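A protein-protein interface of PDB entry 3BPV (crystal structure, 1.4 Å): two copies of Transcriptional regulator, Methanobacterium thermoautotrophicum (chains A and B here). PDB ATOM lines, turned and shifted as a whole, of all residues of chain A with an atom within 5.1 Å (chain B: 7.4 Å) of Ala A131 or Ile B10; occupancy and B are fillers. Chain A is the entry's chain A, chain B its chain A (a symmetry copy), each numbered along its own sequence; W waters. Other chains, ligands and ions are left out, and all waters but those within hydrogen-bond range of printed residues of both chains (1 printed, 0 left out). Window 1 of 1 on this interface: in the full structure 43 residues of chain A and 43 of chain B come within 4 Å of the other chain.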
ATOM      1  N   LEU A   7      37.437  12.918 -10.429  1.00  0.00           N
ATOM      2  CA  LEU A   7      36.299  12.030 -10.216  1.00  0.00           C
ATOM      3  C   LEU A   7      36.768  10.582 -10.165  1.00  0.00           C
ATOM      4  O   LEU A   7      36.239   9.769  -9.397  1.00  0.00           O
ATOM      5  CB  LEU A   7      35.257  12.208 -11.327  1.00  0.00           C
ATOM      6  CG  LEU A   7      34.619  13.601 -11.435  1.00  0.00           C
ATOM      7  CD1 LEU A   7      33.533  13.573 -12.509  1.00  0.00           C
ATOM      8  CD2 LEU A   7      34.040  14.026 -10.094  1.00  0.00           C
ATOM      9  N   MET A 126      24.961  19.822  -7.105  1.00  0.00           N
ATOM     10  CA  MET A 126      25.730  20.110  -8.303  1.00  0.00           C
ATOM     11  C   MET A 126      25.934  18.842  -9.109  1.00  0.00           C
ATOM     12  O   MET A 126      25.861  18.865 -10.332  1.00  0.00           O
ATOM     13  CB  MET A 126      27.075  20.745  -7.948  1.00  0.00           C
ATOM     14  CG  MET A 126      26.932  22.168  -7.444  1.00  0.00           C
ATOM     15  SD  MET A 126      28.518  23.001  -7.296  1.00  0.00           S
ATOM     16  CE  MET A 126      29.161  22.273  -5.820  1.00  0.00           C
ATOM     17  N   CYS A 127      26.169  17.723  -8.435  1.00  0.00           N
ATOM     18  CA  CYS A 127      26.366  16.463  -9.145  1.00  0.00           C
ATOM     19  C   CYS A 127      25.105  16.062  -9.881  1.00  0.00           C
ATOM     20  O   CYS A 127      25.168  15.531 -10.988  1.00  0.00           O
ATOM     21  CB  CYS A 127      26.759  15.332  -8.190  1.00  0.00           C
ATOM     22  SG  CYS A 127      27.791  14.091  -8.984  1.00  0.00           S
ATOM     23  N   ARG A 128      23.954  16.291  -9.254  1.00  0.00           N
ATOM     24  CA  ARG A 128      22.690  15.959  -9.896  1.00  0.00           C
ATOM     25  C   ARG A 128      22.548  16.796 -11.161  1.00  0.00           C
ATOM     26  O   ARG A 128      22.163  16.278 -12.204  1.00  0.00           O
ATOM     27  CB  ARG A 128      21.510  16.229  -8.960  1.00  0.00           C
ATOM     28  CG  ARG A 128      20.171  15.843  -9.569  1.00  0.00           C
ATOM     29  CD  ARG A 128      19.002  16.218  -8.675  1.00  0.00           C
ATOM     30  NE  ARG A 128      18.975  15.463  -7.426  1.00  0.00           N
ATOM     31  CZ  ARG A 128      17.975  15.516  -6.550  1.00  0.00           C
ATOM     32  NH1 ARG A 128      16.924  16.292  -6.787  1.00  0.00           N
ATOM     33  NH2 ARG A 128      18.022  14.794  -5.439  1.00  0.00           N
ATOM     34  N   ARG A 129      22.854  18.090 -11.069  1.00  0.00           N
ATOM     35  CA  ARG A 129      22.775  18.965 -12.236  1.00  0.00           C
ATOM     36  C   ARG A 129      23.733  18.524 -13.339  1.00  0.00           C
ATOM     37  O   ARG A 129      23.379  18.544 -14.519  1.00  0.00           O
ATOM     38  CB  ARG A 129      23.080  20.404 -11.839  1.00  0.00           C
ATOM     39  CG  ARG A 129      21.977  21.047 -11.034  1.00  0.00           C
ATOM     40  CD  ARG A 129      22.457  22.326 -10.388  1.00  0.00           C
ATOM     41  NE  ARG A 129      22.905  23.310 -11.368  1.00  0.00           N
ATOM     42  CZ  ARG A 129      23.651  24.365 -11.062  1.00  0.00           C
ATOM     43  NH1 ARG A 129      24.027  24.563  -9.803  1.00  0.00           N
ATOM     44  NH2 ARG A 129      24.032  25.212 -12.009  1.00  0.00           N
ATOM     45  N   LEU A 130      24.948  18.133 -12.969  1.00  0.00           N
ATOM     46  CA  LEU A 130      25.913  17.686 -13.964  1.00  0.00           C
ATOM     47  C   LEU A 130      25.474  16.348 -14.565  1.00  0.00           C
ATOM     48  O   LEU A 130      25.662  16.106 -15.753  1.00  0.00           O
ATOM     49  CB  LEU A 130      27.299  17.565 -13.334  1.00  0.00           C
ATOM     50  CG  LEU A 130      27.884  18.895 -12.857  1.00  0.00           C
ATOM     51  CD1 LEU A 130      29.110  18.625 -12.002  1.00  0.00           C
ATOM     52  CD2 LEU A 130      28.243  19.768 -14.064  1.00  0.00           C
ATOM     53  N   ALA A 131      24.884  15.479 -13.748  1.00  0.00           N
ATOM     54  CA  ALA A 131      24.418  14.187 -14.243  1.00  0.00           C
ATOM     55  C   ALA A 131      23.301  14.415 -15.256  1.00  0.00           C
ATOM     56  O   ALA A 131      23.212  13.711 -16.260  1.00  0.00           O
ATOM     57  CB  ALA A 131      23.912  13.325 -13.089  1.00  0.00           C
ATOM     58  N   GLU A 132      22.445  15.392 -14.978  1.00  0.00           N
ATOM     59  CA  GLU A 132      21.350  15.710 -15.890  1.00  0.00           C
ATOM     60  C   GLU A 132      21.915  16.181 -17.231  1.00  0.00           C
ATOM     61  O   GLU A 132      21.394  15.829 -18.288  1.00  0.00           O
ATOM     62  CB  GLU A 132      20.446  16.780 -15.275  1.00  0.00           C
ATOM     63  CG  GLU A 132      19.806  16.338 -13.961  1.00  0.00           C
ATOM     64  CD  GLU A 132      19.027  17.445 -13.284  1.00  0.00           C
ATOM     65  OE1 GLU A 132      19.527  18.589 -13.249  1.00  0.00           O
ATOM     66  OE2 GLU A 132      17.918  17.170 -12.775  1.00  0.00           O
ATOM     67  N   GLU A 133      22.978  16.980 -17.193  1.00  0.00           N
ATOM     68  CA  GLU A 133      23.612  17.450 -18.420  1.00  0.00           C
ATOM     69  C   GLU A 133      24.274  16.265 -19.125  1.00  0.00           C
ATOM     70  O   GLU A 133      24.225  16.144 -20.348  1.00  0.00           O
ATOM     71  CB  GLU A 133      24.674  18.502 -18.101  1.00  0.00           C
ATOM     72  CG  GLU A 133      25.366  19.076 -19.332  1.00  0.00           C
ATOM     73  CD  GLU A 133      24.469  20.001 -20.132  1.00  0.00           C
ATOM     74  OE1 GLU A 133      24.061  21.045 -19.585  1.00  0.00           O
ATOM     75  OE2 GLU A 133      24.177  19.687 -21.305  1.00  0.00           O
ATOM     76  N   ALA A 134      24.887  15.385 -18.343  1.00  0.00           N
ATOM     77  CA  ALA A 134      25.559  14.215 -18.891  1.00  0.00           C
ATOM     78  C   ALA A 134      24.597  13.334 -19.668  1.00  0.00           C
ATOM     79  O   ALA A 134      24.964  12.773 -20.699  1.00  0.00           O
ATOM     80  CB  ALA A 134      26.220  13.412 -17.766  1.00  0.00           C
ATOM     81  N   VAL A 135      23.370  13.206 -19.169  1.00  0.00           N
ATOM     82  CA  VAL A 135      22.370  12.398 -19.853  1.00  0.00           C
ATOM     83  C   VAL A 135      21.995  13.067 -21.177  1.00  0.00           C
ATOM     84  O   VAL A 135      21.838  12.394 -22.199  1.00  0.00           O
ATOM     85  CB  VAL A 135      21.105  12.217 -18.981  1.00  0.00           C
ATOM     86  CG1 VAL A 135      19.991  11.594 -19.803  1.00  0.00           C
ATOM     87  CG2 VAL A 135      21.422  11.324 -17.784  1.00  0.00           C
ATOM     88  N   ILE B   1      19.408   7.872  -5.590  1.00  0.00           N
ATOM     89  CA  ILE B   1      20.692   7.462  -6.225  1.00  0.00           C
ATOM     90  C   ILE B   1      21.890   7.779  -5.332  1.00  0.00           C
ATOM     91  O   ILE B   1      22.069   8.918  -4.900  1.00  0.00           O
ATOM     92  CB  ILE B   1      20.897   8.184  -7.576  1.00  0.00           C
ATOM     93  CG1 ILE B   1      19.729   7.879  -8.518  1.00  0.00           C
ATOM     94  CG2 ILE B   1      22.210   7.747  -8.209  1.00  0.00           C
ATOM     95  CD1 ILE B   1      19.781   8.644  -9.823  1.00  0.00           C
ATOM     96  N   LEU B   3      25.690   8.634  -4.150  1.00  0.00           N
ATOM     97  CA  LEU B   3      26.622   9.584  -4.747  1.00  0.00           C
ATOM     98  C   LEU B   3      27.401   8.938  -5.881  1.00  0.00           C
ATOM     99  O   LEU B   3      27.573   9.527  -6.951  1.00  0.00           O
ATOM    100  CB  LEU B   3      27.610  10.105  -3.703  1.00  0.00           C
ATOM    101  CG  LEU B   3      28.688  11.044  -4.269  1.00  0.00           C
ATOM    102  CD1 LEU B   3      28.042  12.348  -4.728  1.00  0.00           C
ATOM    103  CD2 LEU B   3      29.743  11.316  -3.215  1.00  0.00           C
ATOM    104  N   LYS B   4      27.879   7.722  -5.654  1.00  0.00           N
ATOM    105  CA  LYS B   4      28.656   7.048  -6.679  1.00  0.00           C
ATOM    106  C   LYS B   4      27.860   6.899  -7.969  1.00  0.00           C
ATOM    107  O   LYS B   4      28.426   6.969  -9.058  1.00  0.00           O
ATOM    108  CB  LYS B   4      29.144   5.689  -6.164  1.00  0.00           C
ATOM    109  CG  LYS B   4      30.040   4.924  -7.130  1.00  0.00           C
ATOM    110  CD  LYS B   4      29.231   3.994  -8.000  1.00  0.00           C
ATOM    111  CE  LYS B   4      30.130   3.243  -8.961  1.00  0.00           C
ATOM    112  NZ  LYS B   4      29.356   2.268  -9.775  1.00  0.00           N
ATOM    113  N   GLY B   5      26.549   6.718  -7.845  1.00  0.00           N
ATOM    114  CA  GLY B   5      25.709   6.572  -9.022  1.00  0.00           C
ATOM    115  C   GLY B   5      25.691   7.848  -9.843  1.00  0.00           C
ATOM    116  O   GLY B   5      25.716   7.805 -11.073  1.00  0.00           O
ATOM    117  N   LEU B   6      25.634   8.989  -9.168  1.00  0.00           N
ATOM    118  CA  LEU B   6      25.641  10.267  -9.868  1.00  0.00           C
ATOM    119  C   LEU B   6      26.977  10.462 -10.572  1.00  0.00           C
ATOM    120  O   LEU B   6      27.016  10.882 -11.734  1.00  0.00           O
ATOM    121  CB  LEU B   6      25.407  11.425  -8.895  1.00  0.00           C
ATOM    122  CG  LEU B   6      24.017  11.490  -8.275  1.00  0.00           C
ATOM    123  CD1 LEU B   6      24.000  12.628  -7.269  1.00  0.00           C
ATOM    124  CD2 LEU B   6      22.953  11.692  -9.358  1.00  0.00           C
ATOM    125  N   LEU B   7      28.071  10.161  -9.872  1.00  0.00           N
ATOM    126  CA  LEU B   7      29.404  10.311 -10.445  1.00  0.00           C
ATOM    127  C   LEU B   7      29.564   9.393 -11.649  1.00  0.00           C
ATOM    128  O   LEU B   7      30.213   9.749 -12.639  1.00  0.00           O
ATOM    129  CB  LEU B   7      30.482  10.000  -9.398  1.00  0.00           C
ATOM    130  CG  LEU B   7      30.507  10.915  -8.165  1.00  0.00           C
ATOM    131  CD1 LEU B   7      31.699  10.541  -7.288  1.00  0.00           C
ATOM    132  CD2 LEU B   7      30.585  12.375  -8.588  1.00  0.00           C
ATOM    133  N   SER B   8      28.960   8.215 -11.576  1.00  0.00           N
ATOM    134  CA  SER B   8      29.042   7.259 -12.671  1.00  0.00           C
ATOM    135  C   SER B   8      28.266   7.727 -13.898  1.00  0.00           C
ATOM    136  O   SER B   8      28.670   7.464 -15.032  1.00  0.00           O
ATOM    137  CB  SER B   8      28.544   5.895 -12.201  1.00  0.00           C
ATOM    138  OG  SER B   8      29.500   5.310 -11.331  1.00  0.00           O
ATOM    139  N   ILE B   9      27.151   8.414 -13.685  1.00  0.00           N
ATOM    140  CA  ILE B   9      26.383   8.921 -14.816  1.00  0.00           C
ATOM    141  C   ILE B   9      27.260   9.954 -15.519  1.00  0.00           C
ATOM    142  O   ILE B   9      27.359   9.968 -16.744  1.00  0.00           O
ATOM    143  CB  ILE B   9      25.068   9.578 -14.353  1.00  0.00           C
ATOM    144  CG1 ILE B   9      24.117   8.497 -13.829  1.00  0.00           C
ATOM    145  CG2 ILE B   9      24.439  10.364 -15.492  1.00  0.00           C
ATOM    146  CD1 ILE B   9      22.901   9.046 -13.114  1.00  0.00           C
ATOM    147  N   ILE B  10      27.907  10.809 -14.735  1.00  0.00           N
ATOM    148  CA  ILE B  10      28.788  11.827 -15.290  1.00  0.00           C
ATOM    149  C   ILE B  10      29.937  11.167 -16.057  1.00  0.00           C
ATOM    150  O   ILE B  10      30.233  11.541 -17.190  1.00  0.00           O
ATOM    151  CB  ILE B  10      29.351  12.726 -14.161  1.00  0.00           C
ATOM    152  CG1 ILE B  10      28.202  13.508 -13.510  1.00  0.00           C
ATOM    153  CG2 ILE B  10      30.426  13.668 -14.714  1.00  0.00           C
ATOM    154  CD1 ILE B  10      28.574  14.230 -12.233  1.00  0.00           C
ATOM    155  N   LEU B  11      30.574  10.167 -15.448  1.00  0.00           N
ATOM    156  CA  LEU B  11      31.694   9.479 -16.083  1.00  0.00           C
ATOM    157  C   LEU B  11      31.275   8.703 -17.334  1.00  0.00           C
ATOM    158  O   LEU B  11      32.082   8.489 -18.237  1.00  0.00           O
ATOM    159  CB  LEU B  11      32.384   8.547 -15.072  1.00  0.00           C
ATOM    160  CG  LEU B  11      33.157   9.286 -13.973  1.00  0.00           C
ATOM    161  CD1 LEU B  11      33.540   8.328 -12.849  1.00  0.00           C
ATOM    162  CD2 LEU B  11      34.391   9.935 -14.570  1.00  0.00           C
ATOM    163  N   ARG B  12      30.019   8.278 -17.405  1.00  0.00           N
ATOM    164  CA  ARG B  12      29.575   7.554 -18.590  1.00  0.00           C
ATOM    165  C   ARG B  12      29.519   8.502 -19.785  1.00  0.00           C
ATOM    166  O   ARG B  12      29.771   8.096 -20.927  1.00  0.00           O
ATOM    167  CB  ARG B  12      28.208   6.905 -18.356  1.00  0.00           C
ATOM    168  CG  ARG B  12      28.281   5.591 -17.599  1.00  0.00           C
ATOM    169  CD  ARG B  12      27.012   4.778 -17.780  1.00  0.00           C
ATOM    170  NE  ARG B  12      25.880   5.322 -17.041  1.00  0.00           N
ATOM    171  CZ  ARG B  12      25.697   5.170 -15.733  1.00  0.00           C
ATOM    172  NH1 ARG B  12      26.574   4.488 -15.014  1.00  0.00           N
ATOM    173  NH2 ARG B  12      24.629   5.696 -15.148  1.00  0.00           N
ATOM    174  N   SER B  13      29.199   9.767 -19.533  1.00  0.00           N
ATOM    175  CA  SER B  13      29.136  10.732 -20.620  1.00  0.00           C
ATOM    176  C   SER B  13      30.554  10.961 -21.116  1.00  0.00           C
ATOM    177  O   SER B  13      30.782  11.139 -22.313  1.00  0.00           O
ATOM    178  CB  SER B  13      28.515  12.051 -20.149  1.00  0.00           C
ATOM    179  OG  SER B  13      29.402  12.811 -19.351  1.00  0.00           O
ATOM    180  N   HIS B  14      31.511  10.930 -20.195  1.00  0.00           N
ATOM    181  CA  HIS B  14      32.910  11.120 -20.549  1.00  0.00           C
ATOM    182  C   HIS B  14      33.368   9.961 -21.423  1.00  0.00           C
ATOM    183  O   HIS B  14      34.060  10.159 -22.422  1.00  0.00           O
ATOM    184  CB  HIS B  14      33.761  11.211 -19.274  1.00  0.00           C
ATOM    185  CG  HIS B  14      35.230  11.332 -19.529  1.00  0.00           C
ATOM    186  ND1 HIS B  14      36.042  10.237 -19.727  1.00  0.00           N
ATOM    187  CD2 HIS B  14      36.036  12.417 -19.615  1.00  0.00           C
ATOM    188  CE1 HIS B  14      37.284  10.642 -19.923  1.00  0.00           C
ATOM    189  NE2 HIS B  14      37.307  11.960 -19.861  1.00  0.00           N
ATOM    190  N   ARG B  15      32.959   8.753 -21.058  1.00  0.00           N
ATOM    191  CA  ARG B  15      33.315   7.566 -21.813  1.00  0.00           C
ATOM    192  C   ARG B  15      32.789   7.642 -23.245  1.00  0.00           C
ATOM    193  O   ARG B  15      33.511   7.336 -24.200  1.00  0.00           O
ATOM    194  CB  ARG B  15      32.762   6.328 -21.105  1.00  0.00           C
ATOM    195  CG  ARG B  15      33.128   5.006 -21.751  1.00  0.00           C
ATOM    196  CD  ARG B  15      33.268   3.929 -20.685  1.00  0.00           C
ATOM    197  NE  ARG B  15      32.146   3.952 -19.757  1.00  0.00           N
ATOM    198  CZ  ARG B  15      32.107   3.285 -18.609  1.00  0.00           C
ATOM    199  NH1 ARG B  15      33.135   2.534 -18.238  1.00  0.00           N
ATOM    200  NH2 ARG B  15      31.035   3.367 -17.829  1.00  0.00           N
ATOM    201  N   VAL B  16      31.533   8.048 -23.391  1.00  0.00           N
ATOM    202  CA  VAL B  16      30.934   8.161 -24.717  1.00  0.00           C
ATOM    203  C   VAL B  16      31.613   9.277 -25.513  1.00  0.00           C
ATOM    204  O   VAL B  16      31.891   9.121 -26.702  1.00  0.00           O
ATOM    205  CB  VAL B  16      29.415   8.444 -24.622  1.00  0.00           C
ATOM    206  CG1 VAL B  16      28.847   8.749 -26.004  1.00  0.00           C
ATOM    207  CG2 VAL B  16      28.698   7.239 -24.029  1.00  0.00           C
ATOM    208  N   TRP B 107      34.868  18.412 -23.190  1.00  0.00           N
ATOM    209  CA  TRP B 107      33.867  17.672 -22.433  1.00  0.00           C
ATOM    210  C   TRP B 107      33.453  18.481 -21.202  1.00  0.00           C
ATOM    211  O   TRP B 107      32.267  18.624 -20.909  1.00  0.00           O
ATOM    212  CB  TRP B 107      34.421  16.311 -22.001  1.00  0.00           C
ATOM    213  CG  TRP B 107      33.485  15.557 -21.118  1.00  0.00           C
ATOM    214  CD1 TRP B 107      32.313  14.957 -21.481  1.00  0.00           C
ATOM    215  CD2 TRP B 107      33.612  15.373 -19.703  1.00  0.00           C
ATOM    216  NE1 TRP B 107      31.702  14.413 -20.375  1.00  0.00           N
ATOM    217  CE2 TRP B 107      32.477  14.655 -19.271  1.00  0.00           C
ATOM    218  CE3 TRP B 107      34.574  15.752 -18.756  1.00  0.00           C
ATOM    219  CZ2 TRP B 107      32.276  14.305 -17.932  1.00  0.00           C
ATOM    220  CZ3 TRP B 107      34.373  15.405 -17.422  1.00  0.00           C
ATOM    221  CH2 TRP B 107      33.232  14.689 -17.026  1.00  0.00           C
ATOM    222  N   LEU B 111      29.775  19.940 -20.197  1.00  0.00           N
ATOM    223  CA  LEU B 111      29.169  19.521 -18.941  1.00  0.00           C
ATOM    224  C   LEU B 111      28.763  20.706 -18.060  1.00  0.00           C
ATOM    225  O   LEU B 111      27.710  20.690 -17.426  1.00  0.00           O
ATOM    226  CB  LEU B 111      30.147  18.635 -18.169  1.00  0.00           C
ATOM    227  CG  LEU B 111      29.526  17.792 -17.049  1.00  0.00           C
ATOM    228  CD1 LEU B 111      28.804  16.606 -17.664  1.00  0.00           C
ATOM    229  CD2 LEU B 111      30.594  17.311 -16.090  1.00  0.00           C
ATOM    230  N   PHE B 115      26.411  26.107 -15.671  1.00  0.00           N
ATOM    231  CA  PHE B 115      27.025  26.465 -14.395  1.00  0.00           C
ATOM    232  C   PHE B 115      27.664  27.839 -14.500  1.00  0.00           C
ATOM    233  O   PHE B 115      28.251  28.171 -15.533  1.00  0.00           O
ATOM    234  CB  PHE B 115      28.141  25.478 -14.040  1.00  0.00           C
ATOM    235  CG  PHE B 115      27.703  24.322 -13.189  1.00  0.00           C
ATOM    236  CD1 PHE B 115      26.635  23.523 -13.567  1.00  0.00           C
ATOM    237  CD2 PHE B 115      28.389  24.020 -12.015  1.00  0.00           C
ATOM    238  CE1 PHE B 115      26.249  22.432 -12.789  1.00  0.00           C
ATOM    239  CE2 PHE B 115      28.010  22.928 -11.227  1.00  0.00           C
ATOM    240  CZ  PHE B 115      26.942  22.137 -11.615  1.00  0.00           C
ATOM    241  N   PHE B 123      32.810  23.600  -7.434  1.00  0.00           N
ATOM    242  CA  PHE B 123      32.695  22.169  -7.662  1.00  0.00           C
ATOM    243  C   PHE B 123      34.080  21.557  -7.750  1.00  0.00           C
ATOM    244  O   PHE B 123      34.350  20.531  -7.127  1.00  0.00           O
ATOM    245  CB  PHE B 123      31.921  21.877  -8.955  1.00  0.00           C
ATOM    246  CG  PHE B 123      31.577  20.419  -9.133  1.00  0.00           C
ATOM    247  CD1 PHE B 123      30.581  19.828  -8.357  1.00  0.00           C
ATOM    248  CD2 PHE B 123      32.280  19.624 -10.029  1.00  0.00           C
ATOM    249  CE1 PHE B 123      30.296  18.464  -8.468  1.00  0.00           C
ATOM    250  CE2 PHE B 123      32.001  18.261 -10.146  1.00  0.00           C
ATOM    251  CZ  PHE B 123      31.003  17.679  -9.358  1.00  0.00           C
HETATM  252  O   HOH W   1      25.421  22.199 -17.339  1.00  0.00           O
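The backbone carbonyl oxygen of Ile B10 lies within hydrogen-bond range of the side-chain hydroxyl of Ser B13.
The side-chain hydroxyl (OG) of Ser B13 sits at hydrogen-bond distance from the indole nitrogen (NE1) of Trp B107 (3.0 Å).
O of Met A126 touches CZ of Phe B115, 3.7 Å away.
Met A126 touches Phe B123 (CB to CD1, 3.6 Å).
Cys A127 touches Leu B6 (SG to CB, 3.6 Å).
SG of Cys A127 touches CD1 of Ile B10, 3.3 Å away.
Arg A129 touches Phe B115.
Leu B111 touches Leu A130 (O to CD2, 3.5 Å).
CD1 of Leu A130 touches CZ of Phe B123, 3.4 Å away.
Ile B9 touches Ala A131.
CG of Glu A133 touches O of Leu B111 (3.4 Å).
CB of Ala A134 touches O of Ile B9, 3.8 Å away.
Printed residues of chain B within 4 Å of Met A126: Phe B115 (3.7 Å) and Phe B123 (3.6 Å).
Ala A131 touches just these residues of chain B: Ile B9 and Ile B10.
Of chain A, only Leu A7 (3.8 Å), Cys A127 (3.3 Å), Leu A130 (3.7 Å), Ala A131 (3.9 Å) and Ala A134 (3.9 Å) come within 4 Å of Ile B10.
Of the printed residues of chain A, Leu B111 touches Leu A130 (3.5 Å) and Glu A133 (3.4 Å).
Of the 11 printed residues of chain A, 9 touch a printed residue of chain B.
Of the 19 printed residues of chain B, 8 touch a printed residue of chain A.
Printed residues of chain B that touch a printed residue of chain A: Leu B6, Leu B7, Ile B9, Ile B10, Ser B13, Leu B111, Phe B115 and Phe B123.
Hydrophobic or aromatic side chains of chain B within 4 Å of the printed part of chain A: Leu B6, Leu B7, Ile B9, Ile B10, Leu B111, Phe B115 and Phe B123.
Among the printed residues, no Asp or Glu carboxylate lies within 4 Å of a Lys or Arg side-chain nitrogen of the other chain.
Position printed for both chains: 7.
Water W1 bridges the backbone carbonyl oxygen (O) of Leu B111 and the side-chain carboxylate (OE1) of Glu A133.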
